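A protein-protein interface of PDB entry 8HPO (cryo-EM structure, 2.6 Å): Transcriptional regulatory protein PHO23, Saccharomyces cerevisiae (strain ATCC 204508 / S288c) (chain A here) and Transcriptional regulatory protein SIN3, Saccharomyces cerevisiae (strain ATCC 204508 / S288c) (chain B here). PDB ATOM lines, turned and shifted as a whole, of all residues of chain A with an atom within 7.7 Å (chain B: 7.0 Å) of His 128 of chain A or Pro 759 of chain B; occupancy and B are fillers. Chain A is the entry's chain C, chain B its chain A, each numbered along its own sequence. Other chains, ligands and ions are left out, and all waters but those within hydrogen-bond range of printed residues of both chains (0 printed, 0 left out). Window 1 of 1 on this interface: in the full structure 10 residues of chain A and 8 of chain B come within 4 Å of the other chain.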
ATOM      1  N   LEU A 123       4.669  20.734 -23.173  1.00  0.00           N
ATOM      2  CA  LEU A 123       4.972  21.910 -22.372  1.00  0.00           C
ATOM      3  C   LEU A 123       3.721  22.715 -22.038  1.00  0.00           C
ATOM      4  O   LEU A 123       3.788  23.927 -21.835  1.00  0.00           O
ATOM      5  CB  LEU A 123       6.010  22.786 -23.072  1.00  0.00           C
ATOM      6  CG  LEU A 123       5.837  23.152 -24.539  1.00  0.00           C
ATOM      7  CD1 LEU A 123       5.106  24.478 -24.687  1.00  0.00           C
ATOM      8  CD2 LEU A 123       7.191  23.218 -25.204  1.00  0.00           C
ATOM      9  N   GLY A 124       2.577  22.049 -21.984  1.00  0.00           N
ATOM     10  CA  GLY A 124       1.390  22.621 -21.383  1.00  0.00           C
ATOM     11  C   GLY A 124       0.768  23.776 -22.148  1.00  0.00           C
ATOM     12  O   GLY A 124       1.150  24.129 -23.260  1.00  0.00           O
ATOM     13  N   VAL A 125      -0.215  24.384 -21.488  1.00  0.00           N
ATOM     14  CA  VAL A 125      -1.167  25.297 -22.102  1.00  0.00           C
ATOM     15  C   VAL A 125      -0.758  26.733 -21.770  1.00  0.00           C
ATOM     16  O   VAL A 125       0.058  26.982 -20.882  1.00  0.00           O
ATOM     17  CB  VAL A 125      -2.608  24.997 -21.629  1.00  0.00           C
ATOM     18  CG1 VAL A 125      -3.651  25.796 -22.401  1.00  0.00           C
ATOM     19  CG2 VAL A 125      -2.888  23.510 -21.723  1.00  0.00           C
ATOM     20  N   ASP A 126      -1.329  27.678 -22.506  1.00  0.00           N
ATOM     21  CA  ASP A 126      -1.134  29.095 -22.256  1.00  0.00           C
ATOM     22  C   ASP A 126      -2.262  29.658 -21.395  1.00  0.00           C
ATOM     23  O   ASP A 126      -3.446  29.437 -21.659  1.00  0.00           O
ATOM     24  CB  ASP A 126      -1.049  29.868 -23.571  1.00  0.00           C
ATOM     25  CG  ASP A 126       0.018  29.323 -24.491  1.00  0.00           C
ATOM     26  OD1 ASP A 126       0.917  30.093 -24.890  1.00  0.00           O
ATOM     27  OD2 ASP A 126      -0.040  28.117 -24.808  1.00  0.00           O
ATOM     28  N   ASN A 127      -1.860  30.366 -20.339  1.00  0.00           N
ATOM     29  CA  ASN A 127      -2.705  31.167 -19.457  1.00  0.00           C
ATOM     30  C   ASN A 127      -3.549  30.370 -18.466  1.00  0.00           C
ATOM     31  O   ASN A 127      -4.107  30.973 -17.545  1.00  0.00           O
ATOM     32  CB  ASN A 127      -3.622  32.078 -20.277  1.00  0.00           C
ATOM     33  CG  ASN A 127      -2.857  32.944 -21.252  1.00  0.00           C
ATOM     34  OD1 ASN A 127      -2.568  32.530 -22.374  1.00  0.00           O
ATOM     35  ND2 ASN A 127      -2.516  34.155 -20.826  1.00  0.00           N
ATOM     36  N   HIS A 128      -3.695  29.044 -18.656  1.00  0.00           N
ATOM     37  CA  HIS A 128      -3.941  28.096 -17.565  1.00  0.00           C
ATOM     38  C   HIS A 128      -4.816  28.634 -16.441  1.00  0.00           C
ATOM     39  O   HIS A 128      -4.261  29.219 -15.513  1.00  0.00           O
ATOM     40  CB  HIS A 128      -2.672  27.553 -16.922  1.00  0.00           C
ATOM     41  CG  HIS A 128      -2.959  26.451 -15.947  1.00  0.00           C
ATOM     42  ND1 HIS A 128      -2.846  25.118 -16.274  1.00  0.00           N
ATOM     43  CD2 HIS A 128      -3.431  26.484 -14.679  1.00  0.00           C
ATOM     44  CE1 HIS A 128      -3.201  24.380 -15.238  1.00  0.00           C
ATOM     45  NE2 HIS A 128      -3.562  25.186 -14.257  1.00  0.00           N
ATOM     46  N   PRO A 129      -6.143  28.449 -16.460  1.00  0.00           N
ATOM     47  CA  PRO A 129      -7.063  29.246 -15.617  1.00  0.00           C
ATOM     48  C   PRO A 129      -6.521  29.784 -14.296  1.00  0.00           C
ATOM     49  O   PRO A 129      -6.952  30.851 -13.848  1.00  0.00           O
ATOM     50  CB  PRO A 129      -8.207  28.265 -15.339  1.00  0.00           C
ATOM     51  CG  PRO A 129      -8.137  27.255 -16.403  1.00  0.00           C
ATOM     52  CD  PRO A 129      -6.728  27.164 -16.870  1.00  0.00           C
ATOM     53  N   ALA A 130      -5.582  29.083 -13.668  1.00  0.00           N
ATOM     54  CA  ALA A 130      -4.849  29.624 -12.527  1.00  0.00           C
ATOM     55  C   ALA A 130      -3.963  30.766 -13.030  1.00  0.00           C
ATOM     56  O   ALA A 130      -4.196  31.346 -14.094  1.00  0.00           O
ATOM     57  CB  ALA A 130      -4.044  28.530 -11.835  1.00  0.00           C
ATOM     58  N   MET A 131      -3.004  31.194 -12.218  1.00  0.00           N
ATOM     59  CA  MET A 131      -2.014  32.178 -12.642  1.00  0.00           C
ATOM     60  C   MET A 131      -2.606  33.572 -12.820  1.00  0.00           C
ATOM     61  O   MET A 131      -1.939  34.467 -13.338  1.00  0.00           O
ATOM     62  CB  MET A 131      -1.313  31.735 -13.936  1.00  0.00           C
ATOM     63  CG  MET A 131       0.052  32.352 -14.193  1.00  0.00           C
ATOM     64  SD  MET A 131       1.043  31.355 -15.313  1.00  0.00           S
ATOM     65  CE  MET A 131       0.854  29.736 -14.576  1.00  0.00           C
ATOM     66  N   HIS A 132      -3.855  33.786 -12.407  1.00  0.00           N
ATOM     67  CA  HIS A 132      -4.356  35.152 -12.304  1.00  0.00           C
ATOM     68  C   HIS A 132      -3.847  35.821 -11.036  1.00  0.00           C
ATOM     69  O   HIS A 132      -3.650  37.042 -11.014  1.00  0.00           O
ATOM     70  CB  HIS A 132      -5.886  35.164 -12.339  1.00  0.00           C
ATOM     71  CG  HIS A 132      -6.526  34.517 -11.150  1.00  0.00           C
ATOM     72  ND1 HIS A 132      -6.735  33.158 -11.064  1.00  0.00           N
ATOM     73  CD2 HIS A 132      -7.006  35.044 -10.000  1.00  0.00           C
ATOM     74  CE1 HIS A 132      -7.315  32.875  -9.911  1.00  0.00           C
ATOM     75  NE2 HIS A 132      -7.490  34.003  -9.247  1.00  0.00           N
ATOM     76  N   LEU B 743       0.969  31.132  -8.269  1.00  0.00           N
ATOM     77  CA  LEU B 743      -0.207  30.550  -8.890  1.00  0.00           C
ATOM     78  C   LEU B 743      -1.235  30.164  -7.836  1.00  0.00           C
ATOM     79  O   LEU B 743      -0.907  29.604  -6.788  1.00  0.00           O
ATOM     80  CB  LEU B 743       0.157  29.343  -9.763  1.00  0.00           C
ATOM     81  CG  LEU B 743       0.892  28.112  -9.241  1.00  0.00           C
ATOM     82  CD1 LEU B 743      -0.056  27.130  -8.609  1.00  0.00           C
ATOM     83  CD2 LEU B 743       1.622  27.445 -10.382  1.00  0.00           C
ATOM     84  N   ASP B 744      -2.489  30.487  -8.134  1.00  0.00           N
ATOM     85  CA  ASP B 744      -3.609  30.259  -7.231  1.00  0.00           C
ATOM     86  C   ASP B 744      -4.050  28.811  -7.369  1.00  0.00           C
ATOM     87  O   ASP B 744      -4.693  28.441  -8.354  1.00  0.00           O
ATOM     88  CB  ASP B 744      -4.748  31.223  -7.550  1.00  0.00           C
ATOM     89  CG  ASP B 744      -6.049  30.821  -6.899  1.00  0.00           C
ATOM     90  OD1 ASP B 744      -6.161  30.932  -5.661  1.00  0.00           O
ATOM     91  OD2 ASP B 744      -6.965  30.400  -7.628  1.00  0.00           O
ATOM     92  N   LEU B 745      -3.724  27.997  -6.375  1.00  0.00           N
ATOM     93  CA  LEU B 745      -3.907  26.556  -6.444  1.00  0.00           C
ATOM     94  C   LEU B 745      -5.356  26.125  -6.293  1.00  0.00           C
ATOM     95  O   LEU B 745      -5.612  24.941  -6.058  1.00  0.00           O
ATOM     96  CB  LEU B 745      -3.058  25.875  -5.371  1.00  0.00           C
ATOM     97  CG  LEU B 745      -1.604  25.595  -5.726  1.00  0.00           C
ATOM     98  CD1 LEU B 745      -0.825  25.230  -4.485  1.00  0.00           C
ATOM     99  CD2 LEU B 745      -1.531  24.481  -6.744  1.00  0.00           C
ATOM    100  N   LEU B 747      -7.671  26.389  -8.759  1.00  0.00           N
ATOM    101  CA  LEU B 747      -8.045  25.817 -10.051  1.00  0.00           C
ATOM    102  C   LEU B 747      -7.035  24.779 -10.527  1.00  0.00           C
ATOM    103  O   LEU B 747      -6.440  24.927 -11.588  1.00  0.00           O
ATOM    104  CB  LEU B 747      -8.196  26.929 -11.084  1.00  0.00           C
ATOM    105  CG  LEU B 747      -9.055  28.168 -10.812  1.00  0.00           C
ATOM    106  CD1 LEU B 747     -10.241  27.855  -9.912  1.00  0.00           C
ATOM    107  CD2 LEU B 747      -8.219  29.292 -10.244  1.00  0.00           C
ATOM    108  N   CYS B 748      -6.824  23.719  -9.749  1.00  0.00           N
ATOM    109  CA  CYS B 748      -5.895  22.662 -10.124  1.00  0.00           C
ATOM    110  C   CYS B 748      -6.431  21.323  -9.645  1.00  0.00           C
ATOM    111  O   CYS B 748      -7.144  21.248  -8.646  1.00  0.00           O
ATOM    112  CB  CYS B 748      -4.491  22.896  -9.553  1.00  0.00           C
ATOM    113  SG  CYS B 748      -3.865  24.585  -9.683  1.00  0.00           S
ATOM    114  N   GLU B 749      -6.072  20.263 -10.365  1.00  0.00           N
ATOM    115  CA  GLU B 749      -6.637  18.952 -10.082  1.00  0.00           C
ATOM    116  C   GLU B 749      -6.129  18.419  -8.754  1.00  0.00           C
ATOM    117  O   GLU B 749      -4.927  18.403  -8.490  1.00  0.00           O
ATOM    118  CB  GLU B 749      -6.296  17.966 -11.194  1.00  0.00           C
ATOM    119  CG  GLU B 749      -6.721  16.543 -10.865  1.00  0.00           C
ATOM    120  CD  GLU B 749      -6.038  15.500 -11.720  1.00  0.00           C
ATOM    121  OE1 GLU B 749      -5.905  14.350 -11.252  1.00  0.00           O
ATOM    122  OE2 GLU B 749      -5.640  15.827 -12.856  1.00  0.00           O
ATOM    123  N   LYS B 756      -2.086  19.025  -5.004  1.00  0.00           N
ATOM    124  CA  LYS B 756      -2.627  19.561  -6.242  1.00  0.00           C
ATOM    125  C   LYS B 756      -1.589  19.459  -7.348  1.00  0.00           C
ATOM    126  O   LYS B 756      -0.389  19.620  -7.106  1.00  0.00           O
ATOM    127  CB  LYS B 756      -3.062  21.019  -6.078  1.00  0.00           C
ATOM    128  CG  LYS B 756      -4.067  21.233  -4.978  1.00  0.00           C
ATOM    129  CD  LYS B 756      -5.321  21.889  -5.501  1.00  0.00           C
ATOM    130  CE  LYS B 756      -6.469  21.695  -4.536  1.00  0.00           C
ATOM    131  NZ  LYS B 756      -6.483  20.310  -4.010  1.00  0.00           N
ATOM    132  N   ARG B 757      -2.062  19.204  -8.563  1.00  0.00           N
ATOM    133  CA  ARG B 757      -1.169  19.025  -9.699  1.00  0.00           C
ATOM    134  C   ARG B 757      -0.701  20.370 -10.239  1.00  0.00           C
ATOM    135  O   ARG B 757      -1.497  21.288 -10.440  1.00  0.00           O
ATOM    136  CB  ARG B 757      -1.874  18.245 -10.801  1.00  0.00           C
ATOM    137  CG  ARG B 757      -1.010  17.985 -12.007  1.00  0.00           C
ATOM    138  CD  ARG B 757      -1.818  17.529 -13.214  1.00  0.00           C
ATOM    139  NE  ARG B 757      -2.384  16.196 -13.035  1.00  0.00           N
ATOM    140  CZ  ARG B 757      -1.679  15.073 -13.070  1.00  0.00           C
ATOM    141  NH1 ARG B 757      -0.371  15.113 -13.276  1.00  0.00           N
ATOM    142  NH2 ARG B 757      -2.282  13.906 -12.896  1.00  0.00           N
ATOM    143  N   LEU B 758       0.555  20.475 -10.478  1.00  0.00           N
ATOM    144  CA  LEU B 758       1.037  21.726 -11.036  1.00  0.00           C
ATOM    145  C   LEU B 758       0.720  21.804 -12.521  1.00  0.00           C
ATOM    146  O   LEU B 758       0.555  20.774 -13.181  1.00  0.00           O
ATOM    147  CB  LEU B 758       2.543  21.844 -10.854  1.00  0.00           C
ATOM    148  CG  LEU B 758       3.091  22.336  -9.523  1.00  0.00           C
ATOM    149  CD1 LEU B 758       4.541  21.929  -9.411  1.00  0.00           C
ATOM    150  CD2 LEU B 758       2.937  23.837  -9.417  1.00  0.00           C
ATOM    151  N   PRO B 759       0.628  23.009 -13.079  1.00  0.00           N
ATOM    152  CA  PRO B 759       0.648  23.132 -14.537  1.00  0.00           C
ATOM    153  C   PRO B 759       1.919  22.513 -15.090  1.00  0.00           C
ATOM    154  O   PRO B 759       2.883  22.270 -14.362  1.00  0.00           O
ATOM    155  CB  PRO B 759       0.609  24.645 -14.764  1.00  0.00           C
ATOM    156  CG  PRO B 759      -0.079  25.166 -13.577  1.00  0.00           C
ATOM    157  CD  PRO B 759       0.360  24.299 -12.430  1.00  0.00           C
ATOM    158  N   LYS B 760       1.923  22.251 -16.395  1.00  0.00           N
ATOM    159  CA  LYS B 760       3.091  21.610 -16.982  1.00  0.00           C
ATOM    160  C   LYS B 760       4.271  22.570 -17.060  1.00  0.00           C
ATOM    161  O   LYS B 760       5.411  22.180 -16.793  1.00  0.00           O
ATOM    162  CB  LYS B 760       2.754  21.059 -18.362  1.00  0.00           C
ATOM    163  CG  LYS B 760       2.006  19.747 -18.344  1.00  0.00           C
ATOM    164  CD  LYS B 760       1.269  19.558 -19.648  1.00  0.00           C
ATOM    165  CE  LYS B 760       0.599  18.210 -19.724  1.00  0.00           C
ATOM    166  NZ  LYS B 760      -0.186  18.085 -20.977  1.00  0.00           N
ATOM    167  N   SER B 761       4.020  23.833 -17.408  1.00  0.00           N
ATOM    168  CA  SER B 761       5.123  24.747 -17.676  1.00  0.00           C
ATOM    169  C   SER B 761       5.900  25.107 -16.421  1.00  0.00           C
ATOM    170  O   SER B 761       7.023  25.608 -16.526  1.00  0.00           O
ATOM    171  CB  SER B 761       4.613  26.019 -18.345  1.00  0.00           C
ATOM    172  OG  SER B 761       4.527  27.080 -17.413  1.00  0.00           O
ATOM    173  N   ASP B 762       5.332  24.877 -15.242  1.00  0.00           N
ATOM    174  CA  ASP B 762       6.029  25.109 -13.988  1.00  0.00           C
ATOM    175  C   ASP B 762       6.774  23.876 -13.506  1.00  0.00           C
ATOM    176  O   ASP B 762       7.222  23.844 -12.358  1.00  0.00           O
ATOM    177  CB  ASP B 762       5.048  25.583 -12.917  1.00  0.00           C
ATOM    178  CG  ASP B 762       4.526  26.979 -13.184  1.00  0.00           C
ATOM    179  OD1 ASP B 762       4.331  27.334 -14.363  1.00  0.00           O
ATOM    180  OD2 ASP B 762       4.322  27.731 -12.214  1.00  0.00           O
ATOM    181  N   THR B 763       6.910  22.859 -14.353  1.00  0.00           N
ATOM    182  CA  THR B 763       7.700  21.677 -14.046  1.00  0.00           C
ATOM    183  C   THR B 763       9.012  21.639 -14.820  1.00  0.00           C
ATOM    184  O   THR B 763       9.782  20.687 -14.669  1.00  0.00           O
ATOM    185  CB  THR B 763       6.886  20.411 -14.325  1.00  0.00           C
ATOM    186  OG1 THR B 763       6.359  20.464 -15.655  1.00  0.00           O
ATOM    187  CG2 THR B 763       5.741  20.300 -13.351  1.00  0.00           C
ATOM    188  N   PHE B 764       9.275  22.650 -15.642  1.00  0.00           N
ATOM    189  CA  PHE B 764      10.546  22.828 -16.329  1.00  0.00           C
ATOM    190  C   PHE B 764      11.373  23.926 -15.668  1.00  0.00           C
ATOM    191  O   PHE B 764      11.993  24.744 -16.346  1.00  0.00           O
ATOM    192  CB  PHE B 764      10.348  23.151 -17.809  1.00  0.00           C
ATOM    193  CG  PHE B 764       9.522  22.150 -18.557  1.00  0.00           C
ATOM    194  CD1 PHE B 764       9.766  20.796 -18.435  1.00  0.00           C
ATOM    195  CD2 PHE B 764       8.518  22.569 -19.406  1.00  0.00           C
ATOM    196  CE1 PHE B 764       9.014  19.882 -19.131  1.00  0.00           C
ATOM    197  CE2 PHE B 764       7.762  21.658 -20.102  1.00  0.00           C
ATOM    198  CZ  PHE B 764       8.012  20.311 -19.964  1.00  0.00           C
ATOM    199  N   ASP B 780       8.173  16.188  -8.670  1.00  0.00           N
ATOM    200  CA  ASP B 780       8.230  17.465  -9.372  1.00  0.00           C
ATOM    201  C   ASP B 780       6.893  18.075  -9.774  1.00  0.00           C
ATOM    202  O   ASP B 780       6.890  19.235 -10.192  1.00  0.00           O
ATOM    203  CB  ASP B 780       9.090  17.310 -10.633  1.00  0.00           C
ATOM    204  CG  ASP B 780      10.121  18.402 -10.772  1.00  0.00           C
ATOM    205  OD1 ASP B 780       9.759  19.584 -10.616  1.00  0.00           O
ATOM    206  OD2 ASP B 780      11.298  18.086 -11.028  1.00  0.00           O
ATOM    207  N   GLU B 781       5.767  17.368  -9.674  1.00  0.00           N
ATOM    208  CA  GLU B 781       4.514  17.872 -10.226  1.00  0.00           C
ATOM    209  C   GLU B 781       3.450  18.165  -9.177  1.00  0.00           C
ATOM    210  O   GLU B 781       2.623  19.057  -9.382  1.00  0.00           O
ATOM    211  CB  GLU B 781       3.954  16.882 -11.248  1.00  0.00           C
ATOM    212  CG  GLU B 781       3.550  15.553 -10.654  1.00  0.00           C
ATOM    213  CD  GLU B 781       4.664  14.543 -10.712  1.00  0.00           C
ATOM    214  OE1 GLU B 781       4.518  13.532 -11.427  1.00  0.00           O
ATOM    215  OE2 GLU B 781       5.693  14.766 -10.045  1.00  0.00           O
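His 128 of chain A touches just these residues of chain B: Leu 747 and Pro 759.
Of chain A, only His 128 comes within 4 Å of Pro 759 of chain B.
Of the printed residues of chain B, His 132 of chain A touches Asp 744 and Leu 747.
Of the printed residues of chain B, Gly 124 of chain A touches Lys 760.
Of the printed residues of chain A, Lys 760 of chain B touches Gly 124.
Printed residues of chain A within 4 Å of Leu 747 of chain B: His 128 and His 132.
Val 125 of chain A touches none of the printed residues of chain B.
The nearest residue of chain B that does not touch His 128 of chain A is Cys 748 of chain B (4.6 Å).
The nearest residue of chain A that does not touch Pro 759 of chain B is Met 131 of chain A (4.8 Å).
Of the 17 printed residues of chain B, 5 touch a printed residue of chain A.
Hydrophobic or aromatic side chains of chain B that line the printed part of chain A: Leu 747, Pro 759 and Phe 764.
Of the 10 printed residues of chain A, 5 touch a printed residue of chain B.
Printed residues of chain A that touch a printed residue of chain B: Leu 123, Gly 124, His 128, Ala 130 and His 132.
Along chain A the printed residues that touch a printed residue of chain B span positions 123 to 132.
Among the printed residues, pairs that only touch across the chains: Leu 123 of chain A with Phe 764 of chain B (3.6 Å), Gly 124 of chain A with Lys 760 of chain B (3.5 Å), His 128 of chain A with Leu 747 of chain B (3.9 Å), His 128 of chain A with Pro 759 of chain B (3.5 Å), Ala 130 of chain A with Asp 744 of chain B (3.5 Å), His 132 of chain A with Asp 744 of chain B (3.4 Å) and His 132 of chain A with Leu 747 of chain B (3.7 Å).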
